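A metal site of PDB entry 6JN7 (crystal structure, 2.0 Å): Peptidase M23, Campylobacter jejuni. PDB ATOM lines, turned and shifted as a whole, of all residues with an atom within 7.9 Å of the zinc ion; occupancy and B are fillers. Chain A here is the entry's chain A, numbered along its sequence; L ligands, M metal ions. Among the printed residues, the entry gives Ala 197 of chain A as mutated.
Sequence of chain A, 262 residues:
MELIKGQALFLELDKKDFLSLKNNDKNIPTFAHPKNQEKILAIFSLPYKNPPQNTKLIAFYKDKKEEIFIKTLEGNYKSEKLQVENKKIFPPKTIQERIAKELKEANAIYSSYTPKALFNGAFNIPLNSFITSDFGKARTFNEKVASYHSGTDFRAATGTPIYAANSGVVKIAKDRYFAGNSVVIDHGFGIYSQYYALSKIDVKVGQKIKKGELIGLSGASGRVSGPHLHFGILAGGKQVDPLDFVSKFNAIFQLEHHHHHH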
ATOM      1  N   GLU A  80     -16.569  31.876  24.846  1.00  0.00           N
ATOM      2  CA  GLU A  80     -15.353  31.934  25.635  1.00  0.00           C
ATOM      3  C   GLU A  80     -14.168  32.123  24.691  1.00  0.00           C
ATOM      4  O   GLU A  80     -14.216  31.729  23.516  1.00  0.00           O
ATOM      5  CB  GLU A  80     -15.153  30.659  26.444  1.00  0.00           C
ATOM      6  CG  GLU A  80     -15.155  29.374  25.618  1.00  0.00           C
ATOM      7  CD  GLU A  80     -15.161  28.106  26.505  1.00  0.00           C
ATOM      8  OE1 GLU A  80     -14.986  28.240  27.743  1.00  0.00           O
ATOM      9  OE2 GLU A  80     -15.360  26.986  25.987  1.00  0.00           O
ATOM     10  N   THR A 132     -17.051  23.573  33.338  1.00  0.00           N
ATOM     11  CA  THR A 132     -16.102  24.602  32.903  1.00  0.00           C
ATOM     12  C   THR A 132     -16.427  25.120  31.512  1.00  0.00           C
ATOM     13  O   THR A 132     -16.071  26.254  31.185  1.00  0.00           O
ATOM     14  CB  THR A 132     -14.676  24.069  32.925  1.00  0.00           C
ATOM     15  OG1 THR A 132     -14.603  22.877  32.127  1.00  0.00           O
ATOM     16  CG2 THR A 132     -14.231  23.767  34.359  1.00  0.00           C
ATOM     17  N   SER A 133     -17.095  24.325  30.683  1.00  0.00           N
ATOM     18  CA  SER A 133     -17.479  24.769  29.355  1.00  0.00           C
ATOM     19  C   SER A 133     -18.645  23.903  28.915  1.00  0.00           C
ATOM     20  O   SER A 133     -18.481  22.696  28.725  1.00  0.00           O
ATOM     21  CB  SER A 133     -16.295  24.661  28.384  1.00  0.00           C
ATOM     22  OG  SER A 133     -16.664  25.035  27.070  1.00  0.00           O
ATOM     23  N   ASP A 134     -19.821  24.513  28.767  1.00  0.00           N
ATOM     24  CA  ASP A 134     -21.015  23.753  28.401  1.00  0.00           C
ATOM     25  C   ASP A 134     -21.000  23.437  26.898  1.00  0.00           C
ATOM     26  O   ASP A 134     -20.272  24.046  26.112  1.00  0.00           O
ATOM     27  CB  ASP A 134     -22.274  24.544  28.755  1.00  0.00           C
ATOM     28  CG  ASP A 134     -23.530  23.662  28.818  1.00  0.00           C
ATOM     29  OD1 ASP A 134     -23.412  22.430  28.934  1.00  0.00           O
ATOM     30  OD2 ASP A 134     -24.645  24.227  28.770  1.00  0.00           O
ATOM     31  N   PHE A 135     -21.854  22.479  26.526  1.00  0.00           N
ATOM     32  CA  PHE A 135     -22.042  22.144  25.123  1.00  0.00           C
ATOM     33  C   PHE A 135     -22.485  23.362  24.332  1.00  0.00           C
ATOM     34  O   PHE A 135     -23.347  24.133  24.773  1.00  0.00           O
ATOM     35  CB  PHE A 135     -23.095  21.037  24.959  1.00  0.00           C
ATOM     36  CG  PHE A 135     -23.441  20.752  23.528  1.00  0.00           C
ATOM     37  CD1 PHE A 135     -22.722  19.815  22.791  1.00  0.00           C
ATOM     38  CD2 PHE A 135     -24.470  21.454  22.906  1.00  0.00           C
ATOM     39  CE1 PHE A 135     -23.020  19.574  21.450  1.00  0.00           C
ATOM     40  CE2 PHE A 135     -24.774  21.226  21.562  1.00  0.00           C
ATOM     41  CZ  PHE A 135     -24.051  20.285  20.839  1.00  0.00           C
ATOM     42  N   ARG A 139     -16.421  29.261  20.695  1.00  0.00           N
ATOM     43  CA  ARG A 139     -15.048  29.388  21.152  1.00  0.00           C
ATOM     44  C   ARG A 139     -14.226  30.189  20.159  1.00  0.00           C
ATOM     45  O   ARG A 139     -14.375  30.034  18.947  1.00  0.00           O
ATOM     46  CB  ARG A 139     -14.423  27.997  21.350  1.00  0.00           C
ATOM     47  CG  ARG A 139     -15.043  27.240  22.521  1.00  0.00           C
ATOM     48  CD  ARG A 139     -14.565  25.807  22.573  1.00  0.00           C
ATOM     49  NE  ARG A 139     -14.700  25.253  23.915  1.00  0.00           N
ATOM     50  CZ  ARG A 139     -14.336  24.018  24.232  1.00  0.00           C
ATOM     51  NH1 ARG A 139     -13.828  23.223  23.294  1.00  0.00           N
ATOM     52  NH2 ARG A 139     -14.471  23.598  25.482  1.00  0.00           N
ATOM     53  N   TYR A 148     -16.975  25.590  18.114  1.00  0.00           N
ATOM     54  CA  TYR A 148     -18.005  25.446  19.128  1.00  0.00           C
ATOM     55  C   TYR A 148     -17.718  24.164  19.883  1.00  0.00           C
ATOM     56  O   TYR A 148     -17.105  23.247  19.353  1.00  0.00           O
ATOM     57  CB  TYR A 148     -19.412  25.413  18.510  1.00  0.00           C
ATOM     58  CG  TYR A 148     -19.808  24.105  17.848  1.00  0.00           C
ATOM     59  CD1 TYR A 148     -19.496  23.847  16.510  1.00  0.00           C
ATOM     60  CD2 TYR A 148     -20.523  23.155  18.553  1.00  0.00           C
ATOM     61  CE1 TYR A 148     -19.876  22.638  15.902  1.00  0.00           C
ATOM     62  CE2 TYR A 148     -20.896  21.963  17.961  1.00  0.00           C
ATOM     63  CZ  TYR A 148     -20.583  21.709  16.648  1.00  0.00           C
ATOM     64  OH  TYR A 148     -20.996  20.510  16.125  1.00  0.00           O
ATOM     65  N   HIS A 149     -18.167  24.125  21.137  1.00  0.00           N
ATOM     66  CA  HIS A 149     -17.870  22.985  22.003  1.00  0.00           C
ATOM     67  C   HIS A 149     -18.826  21.839  21.682  1.00  0.00           C
ATOM     68  O   HIS A 149     -20.046  21.990  21.768  1.00  0.00           O
ATOM     69  CB  HIS A 149     -17.994  23.406  23.465  1.00  0.00           C
ATOM     70  CG  HIS A 149     -17.441  22.417  24.435  1.00  0.00           C
ATOM     71  ND1 HIS A 149     -17.754  22.425  25.772  1.00  0.00           N
ATOM     72  CD2 HIS A 149     -16.569  21.390  24.253  1.00  0.00           C
ATOM     73  CE1 HIS A 149     -17.099  21.440  26.384  1.00  0.00           C
ATOM     74  NE2 HIS A 149     -16.377  20.811  25.481  1.00  0.00           N
ATOM     75  N   SER A 150     -18.273  20.672  21.303  1.00  0.00           N
ATOM     76  CA  SER A 150     -19.106  19.552  20.882  1.00  0.00           C
ATOM     77  C   SER A 150     -19.442  18.585  22.012  1.00  0.00           C
ATOM     78  O   SER A 150     -20.040  17.533  21.767  1.00  0.00           O
ATOM     79  CB  SER A 150     -18.409  18.780  19.742  1.00  0.00           C
ATOM     80  OG  SER A 150     -17.266  18.126  20.272  1.00  0.00           O
ATOM     81  N   GLY A 151     -19.033  18.900  23.239  1.00  0.00           N
ATOM     82  CA  GLY A 151     -19.421  18.115  24.402  1.00  0.00           C
ATOM     83  C   GLY A 151     -19.530  19.026  25.616  1.00  0.00           C
ATOM     84  O   GLY A 151     -19.640  20.245  25.456  1.00  0.00           O
ATOM     85  N   THR A 152     -19.469  18.470  26.816  1.00  0.00           N
ATOM     86  CA  THR A 152     -19.571  19.251  28.045  1.00  0.00           C
ATOM     87  C   THR A 152     -18.368  18.935  28.931  1.00  0.00           C
ATOM     88  O   THR A 152     -18.022  17.766  29.104  1.00  0.00           O
ATOM     89  CB  THR A 152     -20.887  18.941  28.763  1.00  0.00           C
ATOM     90  OG1 THR A 152     -21.948  19.385  27.913  1.00  0.00           O
ATOM     91  CG2 THR A 152     -20.983  19.661  30.118  1.00  0.00           C
ATOM     92  N   ASP A 153     -17.709  19.981  29.431  1.00  0.00           N
ATOM     93  CA  ASP A 153     -16.494  19.829  30.223  1.00  0.00           C
ATOM     94  C   ASP A 153     -16.810  20.026  31.703  1.00  0.00           C
ATOM     95  O   ASP A 153     -17.444  21.013  32.077  1.00  0.00           O
ATOM     96  CB  ASP A 153     -15.436  20.852  29.804  1.00  0.00           C
ATOM     97  CG  ASP A 153     -14.844  20.570  28.440  1.00  0.00           C
ATOM     98  OD1 ASP A 153     -15.021  19.445  27.922  1.00  0.00           O
ATOM     99  OD2 ASP A 153     -14.200  21.510  27.902  1.00  0.00           O
ATOM    100  N   PHE A 154     -16.306  19.112  32.524  1.00  0.00           N
ATOM    101  CA  PHE A 154     -16.495  19.110  33.978  1.00  0.00           C
ATOM    102  C   PHE A 154     -15.143  19.292  34.637  1.00  0.00           C
ATOM    103  O   PHE A 154     -14.205  18.531  34.367  1.00  0.00           O
ATOM    104  CB  PHE A 154     -17.108  17.788  34.464  1.00  0.00           C
ATOM    105  CG  PHE A 154     -18.461  17.466  33.874  1.00  0.00           C
ATOM    106  CD1 PHE A 154     -18.561  16.905  32.606  1.00  0.00           C
ATOM    107  CD2 PHE A 154     -19.620  17.696  34.593  1.00  0.00           C
ATOM    108  CE1 PHE A 154     -19.803  16.591  32.057  1.00  0.00           C
ATOM    109  CE2 PHE A 154     -20.870  17.391  34.063  1.00  0.00           C
ATOM    110  CZ  PHE A 154     -20.965  16.831  32.787  1.00  0.00           C
ATOM    111  N   ALA A 179      -8.433  15.390  20.951  1.00  0.00           N
ATOM    112  CA  ALA A 179      -8.974  15.340  22.302  1.00  0.00           C
ATOM    113  C   ALA A 179      -8.296  14.288  23.199  1.00  0.00           C
ATOM    114  O   ALA A 179      -8.794  14.013  24.288  1.00  0.00           O
ATOM    115  CB  ALA A 179     -10.478  15.082  22.244  1.00  0.00           C
ATOM    116  N   TYR A 196     -13.405  12.130  26.769  1.00  0.00           N
ATOM    117  CA  TYR A 196     -12.141  12.556  26.195  1.00  0.00           C
ATOM    118  C   TYR A 196     -11.268  13.227  27.247  1.00  0.00           C
ATOM    119  O   TYR A 196     -11.703  13.485  28.375  1.00  0.00           O
ATOM    120  CB  TYR A 196     -12.333  13.533  25.015  1.00  0.00           C
ATOM    121  CG  TYR A 196     -13.213  13.063  23.861  1.00  0.00           C
ATOM    122  CD1 TYR A 196     -13.425  11.709  23.615  1.00  0.00           C
ATOM    123  CD2 TYR A 196     -13.805  13.992  23.014  1.00  0.00           C
ATOM    124  CE1 TYR A 196     -14.231  11.297  22.555  1.00  0.00           C
ATOM    125  CE2 TYR A 196     -14.613  13.593  21.944  1.00  0.00           C
ATOM    126  CZ  TYR A 196     -14.813  12.250  21.728  1.00  0.00           C
ATOM    127  OH  TYR A 196     -15.612  11.854  20.686  1.00  0.00           O
ATOM    128  N   ALA A 197     -10.034  13.537  26.853  1.00  0.00           N
ATOM    129  CA  ALA A 197      -9.045  14.249  27.651  1.00  0.00           C
ATOM    130  C   ALA A 197      -8.520  13.405  28.803  1.00  0.00           C
ATOM    131  O   ALA A 197      -7.913  13.939  29.736  1.00  0.00           O
ATOM    132  CB  ALA A 197      -9.586  15.590  28.180  1.00  0.00           C
ATOM    133  N   GLY A 222      -6.755  16.797  26.543  1.00  0.00           N
ATOM    134  CA  GLY A 222      -7.685  17.172  25.497  1.00  0.00           C
ATOM    135  C   GLY A 222      -7.211  18.341  24.650  1.00  0.00           C
ATOM    136  O   GLY A 222      -6.070  18.807  24.738  1.00  0.00           O
ATOM    137  N   ARG A 223      -8.124  18.815  23.807  1.00  0.00           N
ATOM    138  CA  ARG A 223      -7.847  19.963  22.960  1.00  0.00           C
ATOM    139  C   ARG A 223      -7.675  21.231  23.790  1.00  0.00           C
ATOM    140  O   ARG A 223      -6.736  22.007  23.570  1.00  0.00           O
ATOM    141  CB  ARG A 223      -8.973  20.137  21.932  1.00  0.00           C
ATOM    142  CG  ARG A 223      -8.798  21.331  20.974  1.00  0.00           C
ATOM    143  CD  ARG A 223     -10.075  21.594  20.168  1.00  0.00           C
ATOM    144  NE  ARG A 223     -10.195  20.725  18.987  1.00  0.00           N
ATOM    145  CZ  ARG A 223     -10.946  19.624  18.927  1.00  0.00           C
ATOM    146  NH1 ARG A 223     -11.655  19.216  19.975  1.00  0.00           N
ATOM    147  NH2 ARG A 223     -10.982  18.915  17.799  1.00  0.00           N
ATOM    148  N   VAL A 224      -8.563  21.452  24.769  1.00  0.00           N
ATOM    149  CA  VAL A 224      -8.440  22.629  25.632  1.00  0.00           C
ATOM    150  C   VAL A 224      -7.617  22.222  26.834  1.00  0.00           C
ATOM    151  O   VAL A 224      -7.559  21.043  27.199  1.00  0.00           O
ATOM    152  CB  VAL A 224      -9.802  23.210  26.046  1.00  0.00           C
ATOM    153  CG1 VAL A 224     -10.720  23.388  24.837  1.00  0.00           C
ATOM    154  CG2 VAL A 224     -10.455  22.376  27.121  1.00  0.00           C
ATOM    155  N   HIS A 228      -9.893  18.180  33.280  1.00  0.00           N
ATOM    156  CA  HIS A 228     -11.336  18.118  33.124  1.00  0.00           C
ATOM    157  C   HIS A 228     -11.724  16.824  32.434  1.00  0.00           C
ATOM    158  O   HIS A 228     -10.901  16.183  31.773  1.00  0.00           O
ATOM    159  CB  HIS A 228     -11.877  19.326  32.333  1.00  0.00           C
ATOM    160  CG  HIS A 228     -11.540  19.288  30.867  1.00  0.00           C
ATOM    161  ND1 HIS A 228     -10.293  19.627  30.379  1.00  0.00           N
ATOM    162  CD2 HIS A 228     -12.288  18.951  29.791  1.00  0.00           C
ATOM    163  CE1 HIS A 228     -10.290  19.504  29.060  1.00  0.00           C
ATOM    164  NE2 HIS A 228     -11.481  19.090  28.682  1.00  0.00           N
ATOM    165  N   LEU A 229     -12.984  16.454  32.599  1.00  0.00           N
ATOM    166  CA  LEU A 229     -13.629  15.431  31.785  1.00  0.00           C
ATOM    167  C   LEU A 229     -14.379  16.131  30.652  1.00  0.00           C
ATOM    168  O   LEU A 229     -15.124  17.098  30.890  1.00  0.00           O
ATOM    169  CB  LEU A 229     -14.602  14.593  32.618  1.00  0.00           C
ATOM    170  CG  LEU A 229     -15.497  13.622  31.814  1.00  0.00           C
ATOM    171  CD1 LEU A 229     -14.683  12.510  31.209  1.00  0.00           C
ATOM    172  CD2 LEU A 229     -16.628  13.045  32.661  1.00  0.00           C
ATOM    173  N   HIS A 230     -14.167  15.682  29.424  1.00  0.00           N
ATOM    174  CA  HIS A 230     -15.028  16.047  28.312  1.00  0.00           C
ATOM    175  C   HIS A 230     -15.985  14.889  28.093  1.00  0.00           C
ATOM    176  O   HIS A 230     -15.552  13.757  27.868  1.00  0.00           O
ATOM    177  CB  HIS A 230     -14.215  16.343  27.048  1.00  0.00           C
ATOM    178  CG  HIS A 230     -15.043  16.488  25.807  1.00  0.00           C
ATOM    179  ND1 HIS A 230     -15.267  17.704  25.199  1.00  0.00           N
ATOM    180  CD2 HIS A 230     -15.688  15.558  25.048  1.00  0.00           C
ATOM    181  CE1 HIS A 230     -16.015  17.525  24.113  1.00  0.00           C
ATOM    182  NE2 HIS A 230     -16.285  16.236  24.013  1.00  0.00           N
ATOM    183  N   PHE A 231     -17.286  15.170  28.190  1.00  0.00           N
ATOM    184  CA  PHE A 231     -18.338  14.168  28.024  1.00  0.00           C
ATOM    185  C   PHE A 231     -19.196  14.559  26.834  1.00  0.00           C
ATOM    186  O   PHE A 231     -19.647  15.700  26.749  1.00  0.00           O
ATOM    187  CB  PHE A 231     -19.195  14.091  29.283  1.00  0.00           C
ATOM    188  CG  PHE A 231     -20.321  13.095  29.213  1.00  0.00           C
ATOM    189  CD1 PHE A 231     -20.077  11.747  28.963  1.00  0.00           C
ATOM    190  CD2 PHE A 231     -21.636  13.494  29.451  1.00  0.00           C
ATOM    191  CE1 PHE A 231     -21.119  10.827  28.937  1.00  0.00           C
ATOM    192  CE2 PHE A 231     -22.686  12.577  29.421  1.00  0.00           C
ATOM    193  CZ  PHE A 231     -22.436  11.240  29.165  1.00  0.00           C
ATOM    194  N   GLY A 232     -19.439  13.604  25.934  1.00  0.00           N
ATOM    195  CA  GLY A 232     -20.210  13.893  24.740  1.00  0.00           C
ATOM    196  C   GLY A 232     -21.230  12.813  24.468  1.00  0.00           C
ATOM    197  O   GLY A 232     -21.099  11.682  24.927  1.00  0.00           O
HETATM  198  O1  LIG L   1     -10.633  17.753  24.357  1.00  0.00           O
HETATM  199  O2  LIG L   1     -10.177  19.040  26.071  1.00  0.00           O
HETATM  200  C1  LIG L   1     -10.972  18.580  25.222  1.00  0.00           C
HETATM  201  C2  LIG L   1     -12.394  19.050  25.244  1.00  0.00           C
HETATM  202  O3  LIG L   1     -12.739  19.488  26.556  1.00  0.00           O
HETATM  203  C3  LIG L   1     -12.565  20.208  24.267  1.00  0.00           C
HETATM  204  O4  LIG L   1     -13.756  20.930  24.584  1.00  0.00           O
HETATM  205  C4  LIG L   1     -12.665  19.676  22.863  1.00  0.00           C
HETATM  206  O5  LIG L   1     -13.098  18.508  22.702  1.00  0.00           O
HETATM  207  O6  LIG L   1     -12.310  20.400  21.918  1.00  0.00           O
HETATM  208 ZN    ZN M   1     -14.684  19.535  25.819  1.00  0.00          ZN
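N of Tyr 196 is in hydrogen-bond range of O of His 230, at 2.9 Å. A ring nitrogen (ND1) of His 149 lies within hydrogen-bond range of the backbone carbonyl oxygen of Asp 134, 3.0 Å away. A ring nitrogen (ND1) of His 149 sits close to the backbone carbonyl oxygen (O) of Ser 133 (3.1 Å). NH2 of Arg 139 sits close to ND1 of His 149 (3.5 Å). O of Asp 153 lies within hydrogen-bond range of N of Thr 132. The backbone NH (N) of Asp 153 sits at hydrogen-bond distance from the backbone carbonyl oxygen (O) of Ser 133. O of Gly 151 is in hydrogen-bond range of ND1 of His 149 (2.9 Å). NH2 of Arg 139 lies within salt-bridge range of OD2 of Asp 153, 3.2 Å away.
ND1 of His 230 is bound to the zinc ion, 2.0 Å away. The zinc ion is bound by O3 of the ligand. O4 of the ligand is bound to the zinc ion (2.1 Å). The side-chain carboxylate (OD1) of Asp 153 binds the zinc ion (2.1 Å). The zinc ion is bound by a ring nitrogen (NE2) of His 149.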
